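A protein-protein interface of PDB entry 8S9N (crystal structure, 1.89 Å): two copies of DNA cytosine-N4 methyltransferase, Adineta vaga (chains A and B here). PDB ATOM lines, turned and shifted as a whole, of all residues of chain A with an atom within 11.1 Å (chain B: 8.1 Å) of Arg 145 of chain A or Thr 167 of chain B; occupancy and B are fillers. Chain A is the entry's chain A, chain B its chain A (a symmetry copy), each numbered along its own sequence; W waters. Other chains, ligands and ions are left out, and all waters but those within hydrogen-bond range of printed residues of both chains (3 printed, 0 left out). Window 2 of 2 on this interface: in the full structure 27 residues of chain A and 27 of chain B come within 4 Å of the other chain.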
ATOM      1  N   THR A 139      -8.394 -12.932   7.711  1.00  0.00           N
ATOM      2  CA  THR A 139      -8.852 -14.116   7.010  1.00  0.00           C
ATOM      3  C   THR A 139      -7.636 -14.946   6.634  1.00  0.00           C
ATOM      4  O   THR A 139      -6.559 -14.408   6.375  1.00  0.00           O
ATOM      5  CB  THR A 139      -9.673 -13.744   5.765  1.00  0.00           C
ATOM      6  OG1 THR A 139     -10.013 -14.928   5.034  1.00  0.00           O
ATOM      7  CG2 THR A 139      -8.886 -12.799   4.870  1.00  0.00           C
ATOM      8  N   ASN A 141      -7.604 -16.542   3.947  1.00  0.00           N
ATOM      9  CA  ASN A 141      -7.591 -16.487   2.488  1.00  0.00           C
ATOM     10  C   ASN A 141      -6.781 -15.265   2.074  1.00  0.00           C
ATOM     11  O   ASN A 141      -7.275 -14.134   2.101  1.00  0.00           O
ATOM     12  CB  ASN A 141      -9.009 -16.444   1.934  1.00  0.00           C
ATOM     13  CG  ASN A 141      -9.038 -16.383   0.417  1.00  0.00           C
ATOM     14  OD1 ASN A 141      -8.010 -16.532  -0.239  1.00  0.00           O
ATOM     15  ND2 ASN A 141     -10.219 -16.170  -0.148  1.00  0.00           N
ATOM     16  N   GLN A 142      -5.530 -15.494   1.690  1.00  0.00           N
ATOM     17  CA  GLN A 142      -4.628 -14.418   1.318  1.00  0.00           C
ATOM     18  C   GLN A 142      -4.430 -14.312  -0.186  1.00  0.00           C
ATOM     19  O   GLN A 142      -3.587 -13.526  -0.633  1.00  0.00           O
ATOM     20  CB  GLN A 142      -3.285 -14.593   2.031  1.00  0.00           C
ATOM     21  CG  GLN A 142      -3.369 -14.264   3.523  1.00  0.00           C
ATOM     22  CD  GLN A 142      -3.827 -12.833   3.774  1.00  0.00           C
ATOM     23  OE1 GLN A 142      -3.407 -11.907   3.081  1.00  0.00           O
ATOM     24  NE2 GLN A 142      -4.696 -12.647   4.760  1.00  0.00           N
ATOM     25  N   ASN A 143      -5.190 -15.080  -0.969  1.00  0.00           N
ATOM     26  CA  ASN A 143      -5.185 -14.984  -2.422  1.00  0.00           C
ATOM     27  C   ASN A 143      -5.221 -13.528  -2.859  1.00  0.00           C
ATOM     28  O   ASN A 143      -6.145 -12.786  -2.515  1.00  0.00           O
ATOM     29  CB  ASN A 143      -6.391 -15.742  -2.990  1.00  0.00           C
ATOM     30  CG  ASN A 143      -6.325 -15.911  -4.498  1.00  0.00           C
ATOM     31  OD1 ASN A 143      -6.131 -14.946  -5.241  1.00  0.00           O
ATOM     32  ND2 ASN A 143      -6.475 -17.152  -4.957  1.00  0.00           N
ATOM     33  N   ALA A 144      -4.204 -13.111  -3.610  1.00  0.00           N
ATOM     34  CA  ALA A 144      -3.994 -11.707  -3.927  1.00  0.00           C
ATOM     35  C   ALA A 144      -4.732 -11.266  -5.185  1.00  0.00           C
ATOM     36  O   ALA A 144      -4.412 -10.208  -5.743  1.00  0.00           O
ATOM     37  CB  ALA A 144      -2.497 -11.421  -4.062  1.00  0.00           C
ATOM     38  N   ARG A 145      -5.699 -12.059  -5.655  1.00  0.00           N
ATOM     39  CA  ARG A 145      -6.537 -11.654  -6.776  1.00  0.00           C
ATOM     40  C   ARG A 145      -7.582 -10.618  -6.384  1.00  0.00           C
ATOM     41  O   ARG A 145      -8.222 -10.045  -7.272  1.00  0.00           O
ATOM     42  CB  ARG A 145      -7.240 -12.868  -7.391  1.00  0.00           C
ATOM     43  CG  ARG A 145      -6.365 -13.741  -8.287  1.00  0.00           C
ATOM     44  CD  ARG A 145      -7.225 -14.763  -9.028  1.00  0.00           C
ATOM     45  NE  ARG A 145      -6.484 -15.586  -9.981  1.00  0.00           N
ATOM     46  CZ  ARG A 145      -5.738 -16.626  -9.637  1.00  0.00           C
ATOM     47  NH1 ARG A 145      -5.529 -16.933  -8.368  1.00  0.00           N
ATOM     48  NH2 ARG A 145      -5.200 -17.383 -10.588  1.00  0.00           N
ATOM     49  N   TYR A 146      -7.763 -10.370  -5.088  1.00  0.00           N
ATOM     50  CA  TYR A 146      -8.756  -9.427  -4.594  1.00  0.00           C
ATOM     51  C   TYR A 146      -8.290  -8.904  -3.245  1.00  0.00           C
ATOM     52  O   TYR A 146      -7.288  -9.363  -2.692  1.00  0.00           O
ATOM     53  CB  TYR A 146     -10.138 -10.081  -4.480  1.00  0.00           C
ATOM     54  CG  TYR A 146     -10.082 -11.544  -4.097  1.00  0.00           C
ATOM     55  CD1 TYR A 146      -9.786 -11.933  -2.796  1.00  0.00           C
ATOM     56  CD2 TYR A 146     -10.315 -12.536  -5.041  1.00  0.00           C
ATOM     57  CE1 TYR A 146      -9.728 -13.275  -2.443  1.00  0.00           C
ATOM     58  CE2 TYR A 146     -10.260 -13.878  -4.700  1.00  0.00           C
ATOM     59  CZ  TYR A 146      -9.968 -14.241  -3.398  1.00  0.00           C
ATOM     60  OH  TYR A 146      -9.913 -15.576  -3.054  1.00  0.00           O
ATOM     61  N   PHE A 147      -9.027  -7.929  -2.721  1.00  0.00           N
ATOM     62  CA  PHE A 147      -8.754  -7.434  -1.380  1.00  0.00           C
ATOM     63  C   PHE A 147      -9.120  -8.498  -0.346  1.00  0.00           C
ATOM     64  O   PHE A 147     -10.032  -9.305  -0.551  1.00  0.00           O
ATOM     65  CB  PHE A 147      -9.512  -6.121  -1.142  1.00  0.00           C
ATOM     66  CG  PHE A 147      -9.013  -4.987  -2.004  1.00  0.00           C
ATOM     67  CD1 PHE A 147      -7.930  -4.226  -1.602  1.00  0.00           C
ATOM     68  CD2 PHE A 147      -9.579  -4.730  -3.244  1.00  0.00           C
ATOM     69  CE1 PHE A 147      -7.438  -3.205  -2.405  1.00  0.00           C
ATOM     70  CE2 PHE A 147      -9.096  -3.708  -4.054  1.00  0.00           C
ATOM     71  CZ  PHE A 147      -8.023  -2.945  -3.635  1.00  0.00           C
ATOM     72  N   ARG A 148      -8.379  -8.515   0.759  1.00  0.00           N
ATOM     73  CA  ARG A 148      -8.530  -9.589   1.733  1.00  0.00           C
ATOM     74  C   ARG A 148      -9.974  -9.632   2.215  1.00  0.00           C
ATOM     75  O   ARG A 148     -10.470  -8.631   2.750  1.00  0.00           O
ATOM     76  CB  ARG A 148      -7.588  -9.390   2.915  1.00  0.00           C
ATOM     77  CG  ARG A 148      -6.126  -9.469   2.554  1.00  0.00           C
ATOM     78  CD  ARG A 148      -5.259  -9.092   3.734  1.00  0.00           C
ATOM     79  NE  ARG A 148      -3.847  -9.293   3.438  1.00  0.00           N
ATOM     80  CZ  ARG A 148      -2.866  -8.584   3.977  1.00  0.00           C
ATOM     81  NH1 ARG A 148      -3.112  -7.598   4.825  1.00  0.00           N
ATOM     82  NH2 ARG A 148      -1.607  -8.872   3.660  1.00  0.00           N
ATOM     83  N   PRO A 149     -10.680 -10.735   2.027  1.00  0.00           N
ATOM     84  CA  PRO A 149     -12.129 -10.758   2.302  1.00  0.00           C
ATOM     85  C   PRO A 149     -12.448 -11.154   3.740  1.00  0.00           C
ATOM     86  O   PRO A 149     -12.936 -12.253   4.035  1.00  0.00           O
ATOM     87  CB  PRO A 149     -12.629 -11.788   1.289  1.00  0.00           C
ATOM     88  CG  PRO A 149     -11.508 -12.795   1.256  1.00  0.00           C
ATOM     89  CD  PRO A 149     -10.224 -11.983   1.390  1.00  0.00           C
ATOM     90  N   GLN B  43      -8.354   1.437 -19.262  1.00  0.00           N
ATOM     91  CA  GLN B  43      -7.912   0.413 -18.320  1.00  0.00           C
ATOM     92  C   GLN B  43      -8.634   0.509 -16.981  1.00  0.00           C
ATOM     93  O   GLN B  43      -8.896  -0.519 -16.348  1.00  0.00           O
ATOM     94  CB  GLN B  43      -6.402   0.497 -18.101  1.00  0.00           C
ATOM     95  CG  GLN B  43      -5.864  -0.528 -17.092  1.00  0.00           C
ATOM     96  CD  GLN B  43      -6.170  -1.966 -17.487  1.00  0.00           C
ATOM     97  OE1 GLN B  43      -6.191  -2.307 -18.669  1.00  0.00           O
ATOM     98  NE2 GLN B  43      -6.420  -2.814 -16.495  1.00  0.00           N
ATOM     99  N   PRO B  97     -10.009  -5.601 -21.839  1.00  0.00           N
ATOM    100  CA  PRO B  97     -10.124  -6.902 -21.165  1.00  0.00           C
ATOM    101  C   PRO B  97      -9.200  -6.951 -19.958  1.00  0.00           C
ATOM    102  O   PRO B  97      -8.015  -6.628 -20.047  1.00  0.00           O
ATOM    103  CB  PRO B  97      -9.708  -7.904 -22.248  1.00  0.00           C
ATOM    104  CG  PRO B  97      -9.940  -7.190 -23.538  1.00  0.00           C
ATOM    105  CD  PRO B  97      -9.627  -5.745 -23.256  1.00  0.00           C
ATOM    106  N   GLY B  98      -9.757  -7.343 -18.819  1.00  0.00           N
ATOM    107  CA  GLY B  98      -9.027  -7.272 -17.575  1.00  0.00           C
ATOM    108  C   GLY B  98      -9.003  -5.905 -16.925  1.00  0.00           C
ATOM    109  O   GLY B  98      -8.354  -5.748 -15.883  1.00  0.00           O
ATOM    110  N   GLY B  99      -9.681  -4.913 -17.502  1.00  0.00           N
ATOM    111  CA  GLY B  99      -9.779  -3.610 -16.873  1.00  0.00           C
ATOM    112  C   GLY B  99     -10.724  -3.627 -15.685  1.00  0.00           C
ATOM    113  O   GLY B  99     -11.424  -4.602 -15.414  1.00  0.00           O
ATOM    114  N   SER B 100     -10.742  -2.510 -14.955  1.00  0.00           N
ATOM    115  CA  SER B 100     -11.517  -2.401 -13.724  1.00  0.00           C
ATOM    116  C   SER B 100     -12.309  -1.103 -13.711  1.00  0.00           C
ATOM    117  O   SER B 100     -11.838  -0.071 -14.196  1.00  0.00           O
ATOM    118  CB  SER B 100     -10.610  -2.453 -12.483  1.00  0.00           C
ATOM    119  OG  SER B 100     -10.069  -3.753 -12.287  1.00  0.00           O
ATOM    120  N   GLU B 127     -19.358  -7.206 -14.880  1.00  0.00           N
ATOM    121  CA  GLU B 127     -19.351  -8.270 -13.889  1.00  0.00           C
ATOM    122  C   GLU B 127     -18.873  -7.696 -12.564  1.00  0.00           C
ATOM    123  O   GLU B 127     -17.755  -7.177 -12.476  1.00  0.00           O
ATOM    124  CB  GLU B 127     -18.452  -9.421 -14.332  1.00  0.00           C
ATOM    125  CG  GLU B 127     -17.934 -10.267 -13.183  1.00  0.00           C
ATOM    126  CD  GLU B 127     -17.155 -11.468 -13.666  1.00  0.00           C
ATOM    127  OE1 GLU B 127     -17.394 -11.888 -14.817  1.00  0.00           O
ATOM    128  OE2 GLU B 127     -16.308 -11.986 -12.906  1.00  0.00           O
ATOM    129  N   TYR B 129     -17.119  -7.811  -9.287  1.00  0.00           N
ATOM    130  CA  TYR B 129     -16.002  -8.635  -8.846  1.00  0.00           C
ATOM    131  C   TYR B 129     -15.868  -8.671  -7.329  1.00  0.00           C
ATOM    132  O   TYR B 129     -15.702  -9.743  -6.748  1.00  0.00           O
ATOM    133  CB  TYR B 129     -14.699  -8.126  -9.481  1.00  0.00           C
ATOM    134  CG  TYR B 129     -13.513  -9.025  -9.227  1.00  0.00           C
ATOM    135  CD1 TYR B 129     -13.466 -10.304  -9.767  1.00  0.00           C
ATOM    136  CD2 TYR B 129     -12.437  -8.597  -8.456  1.00  0.00           C
ATOM    137  CE1 TYR B 129     -12.389 -11.141  -9.541  1.00  0.00           C
ATOM    138  CE2 TYR B 129     -11.351  -9.425  -8.228  1.00  0.00           C
ATOM    139  CZ  TYR B 129     -11.336 -10.694  -8.773  1.00  0.00           C
ATOM    140  OH  TYR B 129     -10.268 -11.525  -8.549  1.00  0.00           O
ATOM    141  N   GLN B 130     -15.924  -7.513  -6.678  1.00  0.00           N
ATOM    142  CA  GLN B 130     -15.874  -7.445  -5.223  1.00  0.00           C
ATOM    143  C   GLN B 130     -16.547  -6.153  -4.792  1.00  0.00           C
ATOM    144  O   GLN B 130     -16.564  -5.171  -5.539  1.00  0.00           O
ATOM    145  CB  GLN B 130     -14.428  -7.505  -4.704  1.00  0.00           C
ATOM    146  CG  GLN B 130     -14.288  -7.725  -3.200  1.00  0.00           C
ATOM    147  CD  GLN B 130     -12.836  -7.910  -2.757  1.00  0.00           C
ATOM    148  OE1 GLN B 130     -11.913  -7.392  -3.383  1.00  0.00           O
ATOM    149  NE2 GLN B 130     -12.636  -8.658  -1.675  1.00  0.00           N
ATOM    150  N   TRP B 156     -16.475  -2.906  -7.287  1.00  0.00           N
ATOM    151  CA  TRP B 156     -15.371  -3.202  -8.195  1.00  0.00           C
ATOM    152  C   TRP B 156     -15.899  -4.107  -9.304  1.00  0.00           C
ATOM    153  O   TRP B 156     -16.160  -5.292  -9.076  1.00  0.00           O
ATOM    154  CB  TRP B 156     -14.227  -3.852  -7.422  1.00  0.00           C
ATOM    155  CG  TRP B 156     -12.997  -4.207  -8.211  1.00  0.00           C
ATOM    156  CD1 TRP B 156     -12.722  -3.890  -9.513  1.00  0.00           C
ATOM    157  CD2 TRP B 156     -11.869  -4.951  -7.731  1.00  0.00           C
ATOM    158  NE1 TRP B 156     -11.494  -4.402  -9.874  1.00  0.00           N
ATOM    159  CE2 TRP B 156     -10.951  -5.052  -8.798  1.00  0.00           C
ATOM    160  CE3 TRP B 156     -11.551  -5.547  -6.505  1.00  0.00           C
ATOM    161  CZ2 TRP B 156      -9.733  -5.720  -8.670  1.00  0.00           C
ATOM    162  CZ3 TRP B 156     -10.347  -6.206  -6.379  1.00  0.00           C
ATOM    163  CH2 TRP B 156      -9.451  -6.290  -7.458  1.00  0.00           C
ATOM    164  N   THR B 158     -15.511  -5.650 -13.378  1.00  0.00           N
ATOM    165  CA  THR B 158     -14.539  -5.966 -14.414  1.00  0.00           C
ATOM    166  C   THR B 158     -15.288  -6.289 -15.703  1.00  0.00           C
ATOM    167  O   THR B 158     -16.507  -6.477 -15.707  1.00  0.00           O
ATOM    168  CB  THR B 158     -13.606  -7.108 -13.984  1.00  0.00           C
ATOM    169  OG1 THR B 158     -12.558  -7.262 -14.952  1.00  0.00           O
ATOM    170  CG2 THR B 158     -14.377  -8.414 -13.836  1.00  0.00           C
ATOM    171  N   LYS B 159     -14.546  -6.343 -16.808  1.00  0.00           N
ATOM    172  CA  LYS B 159     -15.156  -6.436 -18.129  1.00  0.00           C
ATOM    173  C   LYS B 159     -15.611  -7.856 -18.437  1.00  0.00           C
ATOM    174  O   LYS B 159     -14.889  -8.824 -18.187  1.00  0.00           O
ATOM    175  CB  LYS B 159     -14.176  -5.970 -19.206  1.00  0.00           C
ATOM    176  CG  LYS B 159     -14.780  -5.939 -20.601  1.00  0.00           C
ATOM    177  CD  LYS B 159     -13.716  -6.054 -21.679  1.00  0.00           C
ATOM    178  CE  LYS B 159     -14.321  -5.878 -23.059  1.00  0.00           C
ATOM    179  NZ  LYS B 159     -14.687  -4.459 -23.339  1.00  0.00           N
ATOM    180  N   GLU B 164     -18.817 -13.815 -20.357  1.00  0.00           N
ATOM    181  CA  GLU B 164     -17.875 -14.698 -19.689  1.00  0.00           C
ATOM    182  C   GLU B 164     -17.015 -13.883 -18.735  1.00  0.00           C
ATOM    183  O   GLU B 164     -16.767 -12.693 -18.953  1.00  0.00           O
ATOM    184  CB  GLU B 164     -16.997 -15.453 -20.699  1.00  0.00           C
ATOM    185  CG  GLU B 164     -16.275 -16.661 -20.122  1.00  0.00           C
ATOM    186  CD  GLU B 164     -15.815 -17.630 -21.195  1.00  0.00           C
ATOM    187  OE1 GLU B 164     -16.392 -17.609 -22.304  1.00  0.00           O
ATOM    188  OE2 GLU B 164     -14.875 -18.410 -20.932  1.00  0.00           O
ATOM    189  N   SER B 165     -16.565 -14.542 -17.672  1.00  0.00           N
ATOM    190  CA  SER B 165     -15.887 -13.875 -16.574  1.00  0.00           C
ATOM    191  C   SER B 165     -14.443 -13.537 -16.941  1.00  0.00           C
ATOM    192  O   SER B 165     -13.969 -13.799 -18.051  1.00  0.00           O
ATOM    193  CB  SER B 165     -15.942 -14.746 -15.321  1.00  0.00           C
ATOM    194  OG  SER B 165     -15.576 -16.082 -15.618  1.00  0.00           O
ATOM    195  N   THR B 166     -13.742 -12.930 -15.987  1.00  0.00           N
ATOM    196  CA  THR B 166     -12.322 -12.644 -16.122  1.00  0.00           C
ATOM    197  C   THR B 166     -11.743 -12.403 -14.738  1.00  0.00           C
ATOM    198  O   THR B 166     -12.470 -12.231 -13.757  1.00  0.00           O
ATOM    199  CB  THR B 166     -12.059 -11.428 -17.013  1.00  0.00           C
ATOM    200  OG1 THR B 166     -10.645 -11.260 -17.178  1.00  0.00           O
ATOM    201  CG2 THR B 166     -12.617 -10.179 -16.367  1.00  0.00           C
ATOM    202  N   THR B 167     -10.418 -12.401 -14.674  1.00  0.00           N
ATOM    203  CA  THR B 167      -9.735 -11.874 -13.514  1.00  0.00           C
ATOM    204  C   THR B 167      -9.118 -10.534 -13.890  1.00  0.00           C
ATOM    205  O   THR B 167      -8.467 -10.423 -14.939  1.00  0.00           O
ATOM    206  CB  THR B 167      -8.662 -12.860 -12.982  1.00  0.00           C
ATOM    207  OG1 THR B 167      -8.356 -12.555 -11.615  1.00  0.00           O
ATOM    208  CG2 THR B 167      -7.375 -12.848 -13.804  1.00  0.00           C
ATOM    209  N   PRO B 168      -9.397  -9.475 -13.140  1.00  0.00           N
ATOM    210  CA  PRO B 168      -8.853  -8.164 -13.506  1.00  0.00           C
ATOM    211  C   PRO B 168      -7.375  -8.073 -13.175  1.00  0.00           C
ATOM    212  O   PRO B 168      -6.901  -8.658 -12.197  1.00  0.00           O
ATOM    213  CB  PRO B 168      -9.677  -7.189 -12.660  1.00  0.00           C
ATOM    214  CG  PRO B 168     -10.057  -7.987 -11.459  1.00  0.00           C
ATOM    215  CD  PRO B 168     -10.265  -9.404 -11.952  1.00  0.00           C
ATOM    216  N   LYS B 169      -6.646  -7.352 -14.020  1.00  0.00           N
ATOM    217  CA  LYS B 169      -5.306  -6.902 -13.668  1.00  0.00           C
ATOM    218  C   LYS B 169      -5.347  -6.241 -12.298  1.00  0.00           C
ATOM    219  O   LYS B 169      -6.082  -5.272 -12.095  1.00  0.00           O
ATOM    220  CB  LYS B 169      -4.810  -5.923 -14.736  1.00  0.00           C
ATOM    221  CG  LYS B 169      -3.443  -5.311 -14.503  1.00  0.00           C
ATOM    222  CD  LYS B 169      -3.022  -4.501 -15.726  1.00  0.00           C
ATOM    223  CE  LYS B 169      -1.774  -3.669 -15.463  1.00  0.00           C
ATOM    224  NZ  LYS B 169      -0.579  -4.520 -15.181  1.00  0.00           N
ATOM    225  N   PHE B 170      -4.586  -6.781 -11.345  1.00  0.00           N
ATOM    226  CA  PHE B 170      -4.677  -6.305  -9.963  1.00  0.00           C
ATOM    227  C   PHE B 170      -3.366  -6.591  -9.251  1.00  0.00           C
ATOM    228  O   PHE B 170      -2.956  -7.752  -9.158  1.00  0.00           O
ATOM    229  CB  PHE B 170      -5.850  -6.977  -9.240  1.00  0.00           C
ATOM    230  CG  PHE B 170      -6.019  -6.552  -7.799  1.00  0.00           C
ATOM    231  CD1 PHE B 170      -6.252  -5.223  -7.470  1.00  0.00           C
ATOM    232  CD2 PHE B 170      -5.991  -7.491  -6.780  1.00  0.00           C
ATOM    233  CE1 PHE B 170      -6.420  -4.835  -6.149  1.00  0.00           C
ATOM    234  CE2 PHE B 170      -6.164  -7.115  -5.455  1.00  0.00           C
ATOM    235  CZ  PHE B 170      -6.385  -5.778  -5.141  1.00  0.00           C
ATOM    236  N   HIS B 171      -2.722  -5.547  -8.730  1.00  0.00           N
ATOM    237  CA  HIS B 171      -1.426  -5.663  -8.061  1.00  0.00           C
ATOM    238  C   HIS B 171      -1.568  -5.157  -6.631  1.00  0.00           C
ATOM    239  O   HIS B 171      -1.241  -4.009  -6.319  1.00  0.00           O
ATOM    240  CB  HIS B 171      -0.364  -4.893  -8.831  1.00  0.00           C
ATOM    241  CG  HIS B 171      -0.309  -5.250 -10.283  1.00  0.00           C
ATOM    242  ND1 HIS B 171       0.471  -6.279 -10.764  1.00  0.00           N
ATOM    243  CD2 HIS B 171      -0.946  -4.725 -11.356  1.00  0.00           C
ATOM    244  CE1 HIS B 171       0.318  -6.367 -12.074  1.00  0.00           C
ATOM    245  NE2 HIS B 171      -0.539  -5.438 -12.457  1.00  0.00           N
ATOM    246  N   ARG B 172      -2.029  -6.047  -5.754  1.00  0.00           N
ATOM    247  CA  ARG B 172      -2.261  -5.688  -4.360  1.00  0.00           C
ATOM    248  C   ARG B 172      -0.963  -5.357  -3.638  1.00  0.00           C
ATOM    249  O   ARG B 172      -0.964  -4.545  -2.704  1.00  0.00           O
ATOM    250  CB  ARG B 172      -2.977  -6.834  -3.653  1.00  0.00           C
ATOM    251  CG  ARG B 172      -3.658  -6.433  -2.361  1.00  0.00           C
ATOM    252  CD  ARG B 172      -4.461  -7.592  -1.804  1.00  0.00           C
ATOM    253  NE  ARG B 172      -3.610  -8.622  -1.222  1.00  0.00           N
ATOM    254  CZ  ARG B 172      -4.065  -9.755  -0.706  1.00  0.00           C
ATOM    255  NH1 ARG B 172      -5.356 -10.042  -0.704  1.00  0.00           N
ATOM    256  NH2 ARG B 172      -3.203 -10.618  -0.171  1.00  0.00           N
HETATM  257  O   HOH W   1      -2.466  -8.649  -6.614  1.00  0.00           O
HETATM  258  O   HOH W   2      -6.921 -12.267   0.024  1.00  0.00           O
HETATM  259  O   HOH W   3      -7.304 -10.443 -10.004  1.00  0.00           O
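O of Gln 142 of chain A sits at hydrogen-bond distance from NH2 of Arg 172 of chain B, at 3.0 Å. The guanidinium group of Arg 172 of chain B is in hydrogen-bond range of the backbone carbonyl oxygen of Asn 143 of chain A (3.4 Å). OH of Tyr 129 of chain B is in hydrogen-bond range of O of Arg 145 of chain A (2.8 Å). The backbone carbonyl oxygen (O) of Tyr 146 of chain A sits at hydrogen-bond distance from the guanidinium group (NH1) of Arg 172 of chain B, at 2.9 Å. The backbone carbonyl oxygen (O) of Phe 147 of chain A is in hydrogen-bond range of the side-chain amide nitrogen (NE2) of Gln 130 of chain B (2.9 Å).
O of Thr 139 of chain A is in hydrogen-bond range of NE2 of Gln 142 of chain A (3.0 Å). The backbone NH (N) of Asn 143 of chain A is in hydrogen-bond range of the side-chain amide oxygen (OD1) of Asn 141 of chain A (3.3 Å). ND2 of Asn 141 of chain A sits at hydrogen-bond distance from OH of Tyr 146 of chain A (3.0 Å). OE1 of Gln 142 of chain A lies within hydrogen-bond range of NE of Arg 148 of chain A, 2.7 Å away. The side-chain hydroxyl (OG) of Ser 100 of chain B lies within hydrogen-bond range of the indole nitrogen (NE1) of Trp 156 of chain B (2.9 Å). N of Tyr 129 of chain B is in hydrogen-bond range of O of Trp 156 of chain B, at 2.7 Å.
Phe 170 of chain B touches Ala 144 of chain A. Ala 144 of chain A touches Arg 172 of chain B (CA to CZ, 3.8 Å). Trp 156 of chain B touches Arg 145 of chain A (CH2 to O, 3.96 Å). Arg 145 of chain A touches Thr 167 of chain B (CD to OG1, 3.6 Å). Phe 170 of chain B touches Arg 145 of chain A. Tyr 129 of chain B touches Tyr 146 of chain A (OH to CD2, 3.7 Å). Tyr 146 of chain A touches Gln 130 of chain B (CB to OE1, 3.4 Å). Tyr 146 of chain A touches Phe 170 of chain B. Phe 147 of chain A touches Phe 170 of chain B. Arg 148 of chain A touches Arg 172 of chain B.
Of chain B, only Tyr 129, Trp 156, Thr 167 and Phe 170 come within 4 Å of Arg 145 of chain A. Thr 167 of chain B touches just one residue of chain A: Arg 145. Ala 144 of chain A touches two residues of chain B. No residue of chain A comes within 4 Å of Thr 166 of chain B. No residue of chain A comes within 4 Å of Pro 168 of chain B. Of the printed residues of chain B, Arg 148 of chain A touches Arg 172 (3.4 Å). Of the printed residues of chain A, Arg 172 of chain B touches Gln 142 (3.0 Å), Asn 143 (3.4 Å), Ala 144 (3.8 Å), Tyr 146 (2.9 Å) and Arg 148 (3.4 Å). Gly 99 of chain B touches none of the printed residues of chain A.
Of the 10 printed residues of chain A, 7 touch a printed residue of chain B. Among the printed residues, 16 pairs touch across the chains. Among the printed residues, no Asp or Glu carboxylate lies within 4 Å of a Lys or Arg side-chain nitrogen of the other chain.
No position is printed for both chains. Of the 16 pairs that touch across the chains among the printed residues, none has its exchanged pair printed and touching as well.
Water W1 lies within hydrogen-bond range of O of Ala 144 of chain A (2.6 Å), O of Phe 170 of chain B (2.7 Å) and N of Arg 172 of chain B (2.8 Å). Water W2 lies within hydrogen-bond range of O of Asn 143 of chain A, O of Asn 141 of chain A and NH1 of Arg 172 of chain B. Water W3 lies within hydrogen-bond range of O of Pro 168 of chain B (2.9 Å), OG1 of Thr 167 of chain B (2.9 Å), O of Arg 145 of chain A (2.9 Å) and OH of Tyr 129 of chain B (3.5 Å).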
